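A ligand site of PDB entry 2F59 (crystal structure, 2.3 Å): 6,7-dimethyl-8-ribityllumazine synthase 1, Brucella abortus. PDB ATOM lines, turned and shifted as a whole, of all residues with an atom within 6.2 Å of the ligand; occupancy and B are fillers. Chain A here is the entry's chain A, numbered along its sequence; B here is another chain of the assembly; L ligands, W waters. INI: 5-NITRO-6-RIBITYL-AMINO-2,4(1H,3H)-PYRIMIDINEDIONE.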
ATOM      1  N   ALA A  20       1.995 -18.267 -24.387  1.00  0.00           N
ATOM      2  CA  ALA A  20       0.916 -17.553 -23.737  1.00  0.00           C
ATOM      3  C   ALA A  20       0.139 -16.954 -24.921  1.00  0.00           C
ATOM      4  O   ALA A  20       0.572 -15.959 -25.520  1.00  0.00           O
ATOM      5  CB  ALA A  20       1.479 -16.447 -22.853  1.00  0.00           C
ATOM      6  N   ARG A  21      -0.984 -17.569 -25.252  1.00  0.00           N
ATOM      7  CA  ARG A  21      -1.799 -17.113 -26.360  1.00  0.00           C
ATOM      8  C   ARG A  21      -2.835 -16.086 -25.936  1.00  0.00           C
ATOM      9  O   ARG A  21      -3.994 -16.414 -25.697  1.00  0.00           O
ATOM     10  CB  ARG A  21      -2.483 -18.324 -27.022  1.00  0.00           C
ATOM     11  CG  ARG A  21      -3.164 -18.014 -28.349  1.00  0.00           C
ATOM     12  CD  ARG A  21      -3.364 -19.286 -29.149  1.00  0.00           C
ATOM     13  NE  ARG A  21      -2.120 -19.776 -29.754  1.00  0.00           N
ATOM     14  CZ  ARG A  21      -1.637 -19.365 -30.923  1.00  0.00           C
ATOM     15  NH1 ARG A  21      -2.277 -18.449 -31.635  1.00  0.00           N
ATOM     16  NH2 ARG A  21      -0.499 -19.876 -31.391  1.00  0.00           N
ATOM     17  N   PHE A  22      -2.395 -14.837 -25.859  1.00  0.00           N
ATOM     18  CA  PHE A  22      -3.245 -13.730 -25.479  1.00  0.00           C
ATOM     19  C   PHE A  22      -3.651 -13.045 -26.792  1.00  0.00           C
ATOM     20  O   PHE A  22      -4.833 -12.963 -27.119  1.00  0.00           O
ATOM     21  CB  PHE A  22      -2.453 -12.772 -24.582  1.00  0.00           C
ATOM     22  CG  PHE A  22      -3.314 -11.786 -23.838  1.00  0.00           C
ATOM     23  CD1 PHE A  22      -4.172 -12.209 -22.843  1.00  0.00           C
ATOM     24  CD2 PHE A  22      -3.265 -10.432 -24.161  1.00  0.00           C
ATOM     25  CE1 PHE A  22      -4.990 -11.302 -22.151  1.00  0.00           C
ATOM     26  CE2 PHE A  22      -4.079  -9.519 -23.485  1.00  0.00           C
ATOM     27  CZ  PHE A  22      -4.940  -9.951 -22.488  1.00  0.00           C
ATOM     28  N   TYR A  23      -2.660 -12.557 -27.532  1.00  0.00           N
ATOM     29  CA  TYR A  23      -2.906 -11.933 -28.834  1.00  0.00           C
ATOM     30  C   TYR A  23      -2.664 -13.061 -29.830  1.00  0.00           C
ATOM     31  O   TYR A  23      -1.524 -13.366 -30.188  1.00  0.00           O
ATOM     32  CB  TYR A  23      -1.924 -10.785 -29.085  1.00  0.00           C
ATOM     33  CG  TYR A  23      -2.115  -9.630 -28.129  1.00  0.00           C
ATOM     34  CD1 TYR A  23      -1.227  -9.403 -27.086  1.00  0.00           C
ATOM     35  CD2 TYR A  23      -3.205  -8.763 -28.275  1.00  0.00           C
ATOM     36  CE1 TYR A  23      -1.408  -8.341 -26.195  1.00  0.00           C
ATOM     37  CE2 TYR A  23      -3.398  -7.700 -27.399  1.00  0.00           C
ATOM     38  CZ  TYR A  23      -2.499  -7.490 -26.366  1.00  0.00           C
ATOM     39  OH  TYR A  23      -2.684  -6.434 -25.510  1.00  0.00           O
ATOM     40  N   PRO A  51      -3.313 -19.220 -21.336  1.00  0.00           N
ATOM     41  CA  PRO A  51      -4.018 -17.968 -21.594  1.00  0.00           C
ATOM     42  C   PRO A  51      -3.188 -16.691 -21.586  1.00  0.00           C
ATOM     43  O   PRO A  51      -3.462 -15.771 -22.364  1.00  0.00           O
ATOM     44  CB  PRO A  51      -5.105 -17.954 -20.521  1.00  0.00           C
ATOM     45  CG  PRO A  51      -4.529 -18.762 -19.416  1.00  0.00           C
ATOM     46  CD  PRO A  51      -3.828 -19.892 -20.128  1.00  0.00           C
ATOM     47  N   GLY A  52      -2.170 -16.636 -20.734  1.00  0.00           N
ATOM     48  CA  GLY A  52      -1.351 -15.438 -20.658  1.00  0.00           C
ATOM     49  C   GLY A  52       0.053 -15.714 -20.146  1.00  0.00           C
ATOM     50  O   GLY A  52       0.341 -16.804 -19.633  1.00  0.00           O
ATOM     51  N   ALA A  53       0.927 -14.733 -20.291  1.00  0.00           N
ATOM     52  CA  ALA A  53       2.309 -14.869 -19.859  1.00  0.00           C
ATOM     53  C   ALA A  53       2.425 -15.207 -18.385  1.00  0.00           C
ATOM     54  O   ALA A  53       3.372 -15.882 -17.974  1.00  0.00           O
ATOM     55  CB  ALA A  53       3.093 -13.594 -20.174  1.00  0.00           C
ATOM     56  N   LEU A  54       1.472 -14.747 -17.580  1.00  0.00           N
ATOM     57  CA  LEU A  54       1.518 -15.040 -16.151  1.00  0.00           C
ATOM     58  C   LEU A  54       1.525 -16.534 -15.842  1.00  0.00           C
ATOM     59  O   LEU A  54       2.086 -16.940 -14.835  1.00  0.00           O
ATOM     60  CB  LEU A  54       0.365 -14.355 -15.404  1.00  0.00           C
ATOM     61  CG  LEU A  54       0.555 -12.863 -15.139  1.00  0.00           C
ATOM     62  CD1 LEU A  54      -0.585 -12.331 -14.283  1.00  0.00           C
ATOM     63  CD2 LEU A  54       1.875 -12.623 -14.459  1.00  0.00           C
ATOM     64  N   GLU A  55       0.905 -17.364 -16.679  1.00  0.00           N
ATOM     65  CA  GLU A  55       0.962 -18.785 -16.356  1.00  0.00           C
ATOM     66  C   GLU A  55       2.063 -19.590 -17.040  1.00  0.00           C
ATOM     67  O   GLU A  55       2.118 -20.804 -16.898  1.00  0.00           O
ATOM     68  CB  GLU A  55      -0.398 -19.489 -16.563  1.00  0.00           C
ATOM     69  CG  GLU A  55      -1.314 -18.941 -17.598  1.00  0.00           C
ATOM     70  CD  GLU A  55      -2.047 -17.705 -17.140  1.00  0.00           C
ATOM     71  OE1 GLU A  55      -2.043 -17.397 -15.931  1.00  0.00           O
ATOM     72  OE2 GLU A  55      -2.636 -17.034 -18.008  1.00  0.00           O
ATOM     73  N   GLY A  81       5.362 -15.209 -25.575  1.00  0.00           N
ATOM     74  CA  GLY A  81       4.250 -14.382 -25.151  1.00  0.00           C
ATOM     75  C   GLY A  81       4.450 -12.953 -25.592  1.00  0.00           C
ATOM     76  O   GLY A  81       5.529 -12.557 -26.035  1.00  0.00           O
ATOM     77  N   THR A  82       3.396 -12.170 -25.475  1.00  0.00           N
ATOM     78  CA  THR A  82       3.490 -10.787 -25.845  1.00  0.00           C
ATOM     79  C   THR A  82       2.648  -9.928 -24.917  1.00  0.00           C
ATOM     80  O   THR A  82       1.493 -10.246 -24.629  1.00  0.00           O
ATOM     81  CB  THR A  82       3.020 -10.571 -27.282  1.00  0.00           C
ATOM     82  OG1 THR A  82       3.756 -11.439 -28.164  1.00  0.00           O
ATOM     83  CG2 THR A  82       3.236  -9.117 -27.684  1.00  0.00           C
ATOM     84  N   VAL A  83       3.261  -8.863 -24.436  1.00  0.00           N
ATOM     85  CA  VAL A  83       2.588  -7.910 -23.563  1.00  0.00           C
ATOM     86  C   VAL A  83       2.826  -6.535 -24.192  1.00  0.00           C
ATOM     87  O   VAL A  83       3.960  -6.126 -24.395  1.00  0.00           O
ATOM     88  CB  VAL A  83       3.205  -7.921 -22.145  1.00  0.00           C
ATOM     89  CG1 VAL A  83       2.538  -6.855 -21.284  1.00  0.00           C
ATOM     90  CG2 VAL A  83       3.036  -9.285 -21.506  1.00  0.00           C
ATOM     91  N   ILE A  84       1.741  -5.863 -24.531  1.00  0.00           N
ATOM     92  CA  ILE A  84       1.826  -4.538 -25.129  1.00  0.00           C
ATOM     93  C   ILE A  84       1.406  -3.551 -24.060  1.00  0.00           C
ATOM     94  O   ILE A  84       0.316  -3.682 -23.506  1.00  0.00           O
ATOM     95  CB  ILE A  84       0.862  -4.399 -26.338  1.00  0.00           C
ATOM     96  CG1 ILE A  84       1.152  -5.486 -27.370  1.00  0.00           C
ATOM     97  CG2 ILE A  84       1.024  -3.032 -26.970  1.00  0.00           C
ATOM     98  CD1 ILE A  84       0.134  -5.555 -28.481  1.00  0.00           C
ATOM     99  N   HIS A  90      -1.937  -2.735 -16.130  1.00  0.00           N
ATOM    100  CA  HIS A  90      -1.951  -4.195 -16.086  1.00  0.00           C
ATOM    101  C   HIS A  90      -1.108  -4.818 -17.209  1.00  0.00           C
ATOM    102  O   HIS A  90      -1.497  -5.828 -17.792  1.00  0.00           O
ATOM    103  CB  HIS A  90      -3.409  -4.683 -16.191  1.00  0.00           C
ATOM    104  CG  HIS A  90      -3.599  -6.126 -15.848  1.00  0.00           C
ATOM    105  ND1 HIS A  90      -3.095  -7.152 -16.626  1.00  0.00           N
ATOM    106  CD2 HIS A  90      -4.238  -6.718 -14.806  1.00  0.00           C
ATOM    107  CE1 HIS A  90      -3.421  -8.313 -16.083  1.00  0.00           C
ATOM    108  NE2 HIS A  90      -4.111  -8.078 -14.973  1.00  0.00           N
ATOM    109  N   PHE A  91       0.046  -4.229 -17.497  1.00  0.00           N
ATOM    110  CA  PHE A  91       0.893  -4.766 -18.568  1.00  0.00           C
ATOM    111  C   PHE A  91       2.346  -5.031 -18.172  1.00  0.00           C
ATOM    112  O   PHE A  91       2.859  -6.137 -18.369  1.00  0.00           O
ATOM    113  CB  PHE A  91       0.834  -3.854 -19.789  1.00  0.00           C
ATOM    114  CG  PHE A  91      -0.562  -3.603 -20.309  1.00  0.00           C
ATOM    115  CD1 PHE A  91      -1.300  -2.519 -19.865  1.00  0.00           C
ATOM    116  CD2 PHE A  91      -1.128  -4.471 -21.243  1.00  0.00           C
ATOM    117  CE1 PHE A  91      -2.587  -2.285 -20.345  1.00  0.00           C
ATOM    118  CE2 PHE A  91      -2.425  -4.246 -21.728  1.00  0.00           C
ATOM    119  CZ  PHE A  91      -3.154  -3.153 -21.279  1.00  0.00           C
ATOM    120  N   VAL A  94       2.738  -8.090 -15.983  1.00  0.00           N
ATOM    121  CA  VAL A  94       2.732  -9.393 -16.632  1.00  0.00           C
ATOM    122  C   VAL A  94       4.129  -9.769 -17.124  1.00  0.00           C
ATOM    123  O   VAL A  94       4.617 -10.871 -16.850  1.00  0.00           O
ATOM    124  CB  VAL A  94       1.737  -9.423 -17.824  1.00  0.00           C
ATOM    125  CG1 VAL A  94       1.884 -10.736 -18.585  1.00  0.00           C
ATOM    126  CG2 VAL A  94       0.307  -9.265 -17.303  1.00  0.00           C
ATOM    127  N   ILE B 113      -3.338 -21.292 -10.834  1.00  0.00           N
ATOM    128  CA  ILE B 113      -3.843 -20.011 -10.365  1.00  0.00           C
ATOM    129  C   ILE B 113      -4.302 -19.132 -11.509  1.00  0.00           C
ATOM    130  O   ILE B 113      -3.564 -18.884 -12.455  1.00  0.00           O
ATOM    131  CB  ILE B 113      -2.753 -19.213  -9.600  1.00  0.00           C
ATOM    132  CG1 ILE B 113      -2.268 -19.999  -8.382  1.00  0.00           C
ATOM    133  CG2 ILE B 113      -3.331 -17.892  -9.160  1.00  0.00           C
ATOM    134  CD1 ILE B 113      -1.240 -19.250  -7.543  1.00  0.00           C
ATOM    135  N   GLY B 114      -5.551 -18.688 -11.418  1.00  0.00           N
ATOM    136  CA  GLY B 114      -6.096 -17.780 -12.413  1.00  0.00           C
ATOM    137  C   GLY B 114      -5.941 -16.430 -11.767  1.00  0.00           C
ATOM    138  O   GLY B 114      -6.476 -16.186 -10.679  1.00  0.00           O
ATOM    139  N   ASN B 115      -5.186 -15.535 -12.386  1.00  0.00           N
ATOM    140  CA  ASN B 115      -4.968 -14.215 -11.831  1.00  0.00           C
ATOM    141  C   ASN B 115      -5.982 -13.204 -12.327  1.00  0.00           C
ATOM    142  O   ASN B 115      -5.914 -12.724 -13.466  1.00  0.00           O
ATOM    143  CB  ASN B 115      -3.560 -13.724 -12.174  1.00  0.00           C
ATOM    144  CG  ASN B 115      -3.207 -12.459 -11.421  1.00  0.00           C
ATOM    145  OD1 ASN B 115      -4.047 -11.582 -11.241  1.00  0.00           O
ATOM    146  ND2 ASN B 115      -1.948 -12.359 -10.980  1.00  0.00           N
ATOM    147  N   GLY B 116      -6.936 -12.870 -11.462  1.00  0.00           N
ATOM    148  CA  GLY B 116      -7.949 -11.912 -11.807  1.00  0.00           C
ATOM    149  C   GLY B 116      -7.744 -10.619 -11.049  1.00  0.00           C
ATOM    150  O   GLY B 116      -8.707  -9.904 -10.764  1.00  0.00           O
ATOM    151  N   ILE B 117      -6.509 -10.314 -10.695  1.00  0.00           N
ATOM    152  CA  ILE B 117      -6.230  -9.067  -9.986  1.00  0.00           C
ATOM    153  C   ILE B 117      -6.106  -7.959 -11.025  1.00  0.00           C
ATOM    154  O   ILE B 117      -5.088  -7.837 -11.726  1.00  0.00           O
ATOM    155  CB  ILE B 117      -4.940  -9.141  -9.166  1.00  0.00           C
ATOM    156  CG1 ILE B 117      -5.065 -10.246  -8.114  1.00  0.00           C
ATOM    157  CG2 ILE B 117      -4.685  -7.801  -8.511  1.00  0.00           C
ATOM    158  CD1 ILE B 117      -3.794 -10.455  -7.299  1.00  0.00           C
ATOM    159  N   LYS B 137     -12.709  -9.875 -16.895  1.00  0.00           N
ATOM    160  CA  LYS B 137     -11.446 -10.297 -16.328  1.00  0.00           C
ATOM    161  C   LYS B 137     -11.668 -11.462 -15.354  1.00  0.00           C
ATOM    162  O   LYS B 137     -10.879 -12.417 -15.330  1.00  0.00           O
ATOM    163  CB  LYS B 137     -10.780  -9.139 -15.588  1.00  0.00           C
ATOM    164  CG  LYS B 137      -9.411  -9.453 -14.960  1.00  0.00           C
ATOM    165  CD  LYS B 137      -8.330  -9.679 -16.026  1.00  0.00           C
ATOM    166  CE  LYS B 137      -6.929  -9.771 -15.413  1.00  0.00           C
ATOM    167  NZ  LYS B 137      -5.893 -10.045 -16.470  1.00  0.00           N
ATOM    168  N   PHE B 140     -12.156 -14.582 -17.257  1.00  0.00           N
ATOM    169  CA  PHE B 140     -10.874 -14.904 -17.872  1.00  0.00           C
ATOM    170  C   PHE B 140     -10.000 -15.624 -16.849  1.00  0.00           C
ATOM    171  O   PHE B 140      -9.458 -16.695 -17.133  1.00  0.00           O
ATOM    172  CB  PHE B 140     -10.165 -13.628 -18.346  1.00  0.00           C
ATOM    173  CG  PHE B 140      -8.959 -13.896 -19.218  1.00  0.00           C
ATOM    174  CD1 PHE B 140      -9.103 -14.170 -20.582  1.00  0.00           C
ATOM    175  CD2 PHE B 140      -7.675 -13.908 -18.661  1.00  0.00           C
ATOM    176  CE1 PHE B 140      -7.997 -14.463 -21.375  1.00  0.00           C
ATOM    177  CE2 PHE B 140      -6.553 -14.195 -19.454  1.00  0.00           C
ATOM    178  CZ  PHE B 140      -6.720 -14.471 -20.812  1.00  0.00           C
ATOM    179  N   ALA B 141      -9.890 -15.045 -15.663  1.00  0.00           N
ATOM    180  CA  ALA B 141      -9.075 -15.615 -14.586  1.00  0.00           C
ATOM    181  C   ALA B 141      -9.554 -17.008 -14.201  1.00  0.00           C
ATOM    182  O   ALA B 141      -8.762 -17.924 -13.996  1.00  0.00           O
ATOM    183  CB  ALA B 141      -9.090 -14.698 -13.372  1.00  0.00           C
ATOM    184  N   ALA B 144      -8.674 -19.356 -16.903  1.00  0.00           N
ATOM    185  CA  ALA B 144      -7.233 -19.600 -16.870  1.00  0.00           C
ATOM    186  C   ALA B 144      -6.932 -20.650 -15.812  1.00  0.00           C
ATOM    187  O   ALA B 144      -6.125 -21.560 -16.045  1.00  0.00           O
ATOM    188  CB  ALA B 144      -6.487 -18.313 -16.550  1.00  0.00           C
ATOM    189  N   ALA B 145      -7.585 -20.547 -14.661  1.00  0.00           N
ATOM    190  CA  ALA B 145      -7.382 -21.521 -13.598  1.00  0.00           C
ATOM    191  C   ALA B 145      -7.754 -22.906 -14.096  1.00  0.00           C
ATOM    192  O   ALA B 145      -7.050 -23.889 -13.838  1.00  0.00           O
ATOM    193  CB  ALA B 145      -8.236 -21.163 -12.375  1.00  0.00           C
HETATM  194  N1  INI L   1      -1.180 -12.062 -20.906  1.00  0.00           N
HETATM  195  C2  INI L   1      -0.203 -11.920 -21.870  1.00  0.00           C
HETATM  196  O2  INI L   1       0.380 -12.945 -22.184  1.00  0.00           O
HETATM  197  N3  INI L   1       0.024 -10.673 -22.367  1.00  0.00           N
HETATM  198  C4  INI L   1      -0.655  -9.514 -21.982  1.00  0.00           C
HETATM  199  O4  INI L   1      -0.288  -8.464 -22.576  1.00  0.00           O
HETATM  200  C5  INI L   1      -1.762  -9.679 -20.875  1.00  0.00           C
HETATM  201  N5  INI L   1      -2.485  -8.494 -20.440  1.00  0.00           N
HETATM  202  O51 INI L   1      -2.246  -7.438 -20.905  1.00  0.00           O
HETATM  203  O52 INI L   1      -3.338  -8.595 -19.588  1.00  0.00           O
HETATM  204  C6  INI L   1      -1.985 -11.052 -20.361  1.00  0.00           C
HETATM  205  N7  INI L   1      -2.918 -11.486 -19.383  1.00  0.00           N
HETATM  206  C8  INI L   1      -2.378 -11.543 -17.995  1.00  0.00           C
HETATM  207  C9  INI L   1      -2.030 -12.992 -17.457  1.00  0.00           C
HETATM  208  O9  INI L   1      -0.992 -13.417 -18.317  1.00  0.00           O
HETATM  209  C10 INI L   1      -3.112 -14.201 -17.488  1.00  0.00           C
HETATM  210  O10 INI L   1      -3.533 -14.494 -18.770  1.00  0.00           O
HETATM  211  C11 INI L   1      -4.538 -14.096 -16.561  1.00  0.00           C
HETATM  212  O11 INI L   1      -4.315 -12.826 -15.884  1.00  0.00           O
HETATM  213  C12 INI L   1      -4.968 -14.976 -15.291  1.00  0.00           C
HETATM  214  O12 INI L   1      -3.901 -15.844 -15.037  1.00  0.00           O
HETATM  215  O   HOH W   1       1.122 -13.476 -24.560  1.00  0.00           O
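Water W1 lies within hydrogen-bond range of an oxygen (O2) of the ligand, the backbone carbonyl oxygen (O) of Ala 20 and the backbone NH (N) of Thr 82.
Ala 20 touches the ligand.
Phe 22 touches the ligand.
Tyr 23 touches the ligand (CE1 to O4, 3.8 Å).
C of Pro 51 touches O10 of the ligand, 3.6 Å away.
Val 83 touches the ligand (CA to O4, 3.1 Å).
N of Ile 84 touches O4 of the ligand, 3.8 Å away.
CD2 of Phe 91 touches O51 of the ligand (3.2 Å).
Val 94 touches the ligand.
Gly 114 of chain B touches the ligand.
CE2 of Phe 140 of chain B touches O10 of the ligand (3.1 Å).
CB of Ala 144 of chain B touches C12 of the ligand, at 3.9 Å.
Hydrophobic or aromatic side chains within 4 Å of the ligand: Ala 20, Phe 22, Tyr 23, Ala 53, Leu 54, Val 83, His 90, Phe 91, Val 94, Phe 140 of chain B and Ala 144 of chain B.
Of the 26 residues printed, 19 come within 4 Å of the ligand.
The backbone NH (N) of Gly 52 lies within hydrogen-bond range of the side-chain carboxylate (OE2) of Glu 55 (2.8 Å).
The side-chain amide oxygen (OD1) of Asn 115 of chain B sits at hydrogen-bond distance from the backbone NH (N) of Ile 117 of chain B, 2.8 Å away.
A ring nitrogen (NE2) of His 90 lies close to the side-chain amino group (NZ) of Lys 137 of chain B, 3.0 Å away.
NE2 of His 90 sits close to O of Ile 117 of chain B, 3.4 Å away.
The side-chain carboxylate (OE1) of Glu 55 sits at hydrogen-bond distance from an oxygen (O12) of the ligand.
N of Ala 53 is in hydrogen-bond range of O2 of the ligand (2.7 Å).
The backbone carbonyl oxygen (O) of Thr 82 sits at hydrogen-bond distance from a nitrogen (N3) of the ligand (2.7 Å).
N of Leu 54 is in hydrogen-bond range of O9 of the ligand (2.9 Å).
An oxygen (O12) of the ligand is in hydrogen-bond range of the backbone NH of Asn 115 of chain B (3.0 Å).
O of Asn 115 of chain B sits at hydrogen-bond distance from O11 of the ligand, at 2.9 Å.
O10 of the ligand lies close to N of Gly 52 (3.2 Å).
NZ of Lys 137 of chain B sits at hydrogen-bond distance from O11 of the ligand.
ND1 of His 90 sits at hydrogen-bond distance from O52 of the ligand (3.3 Å).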
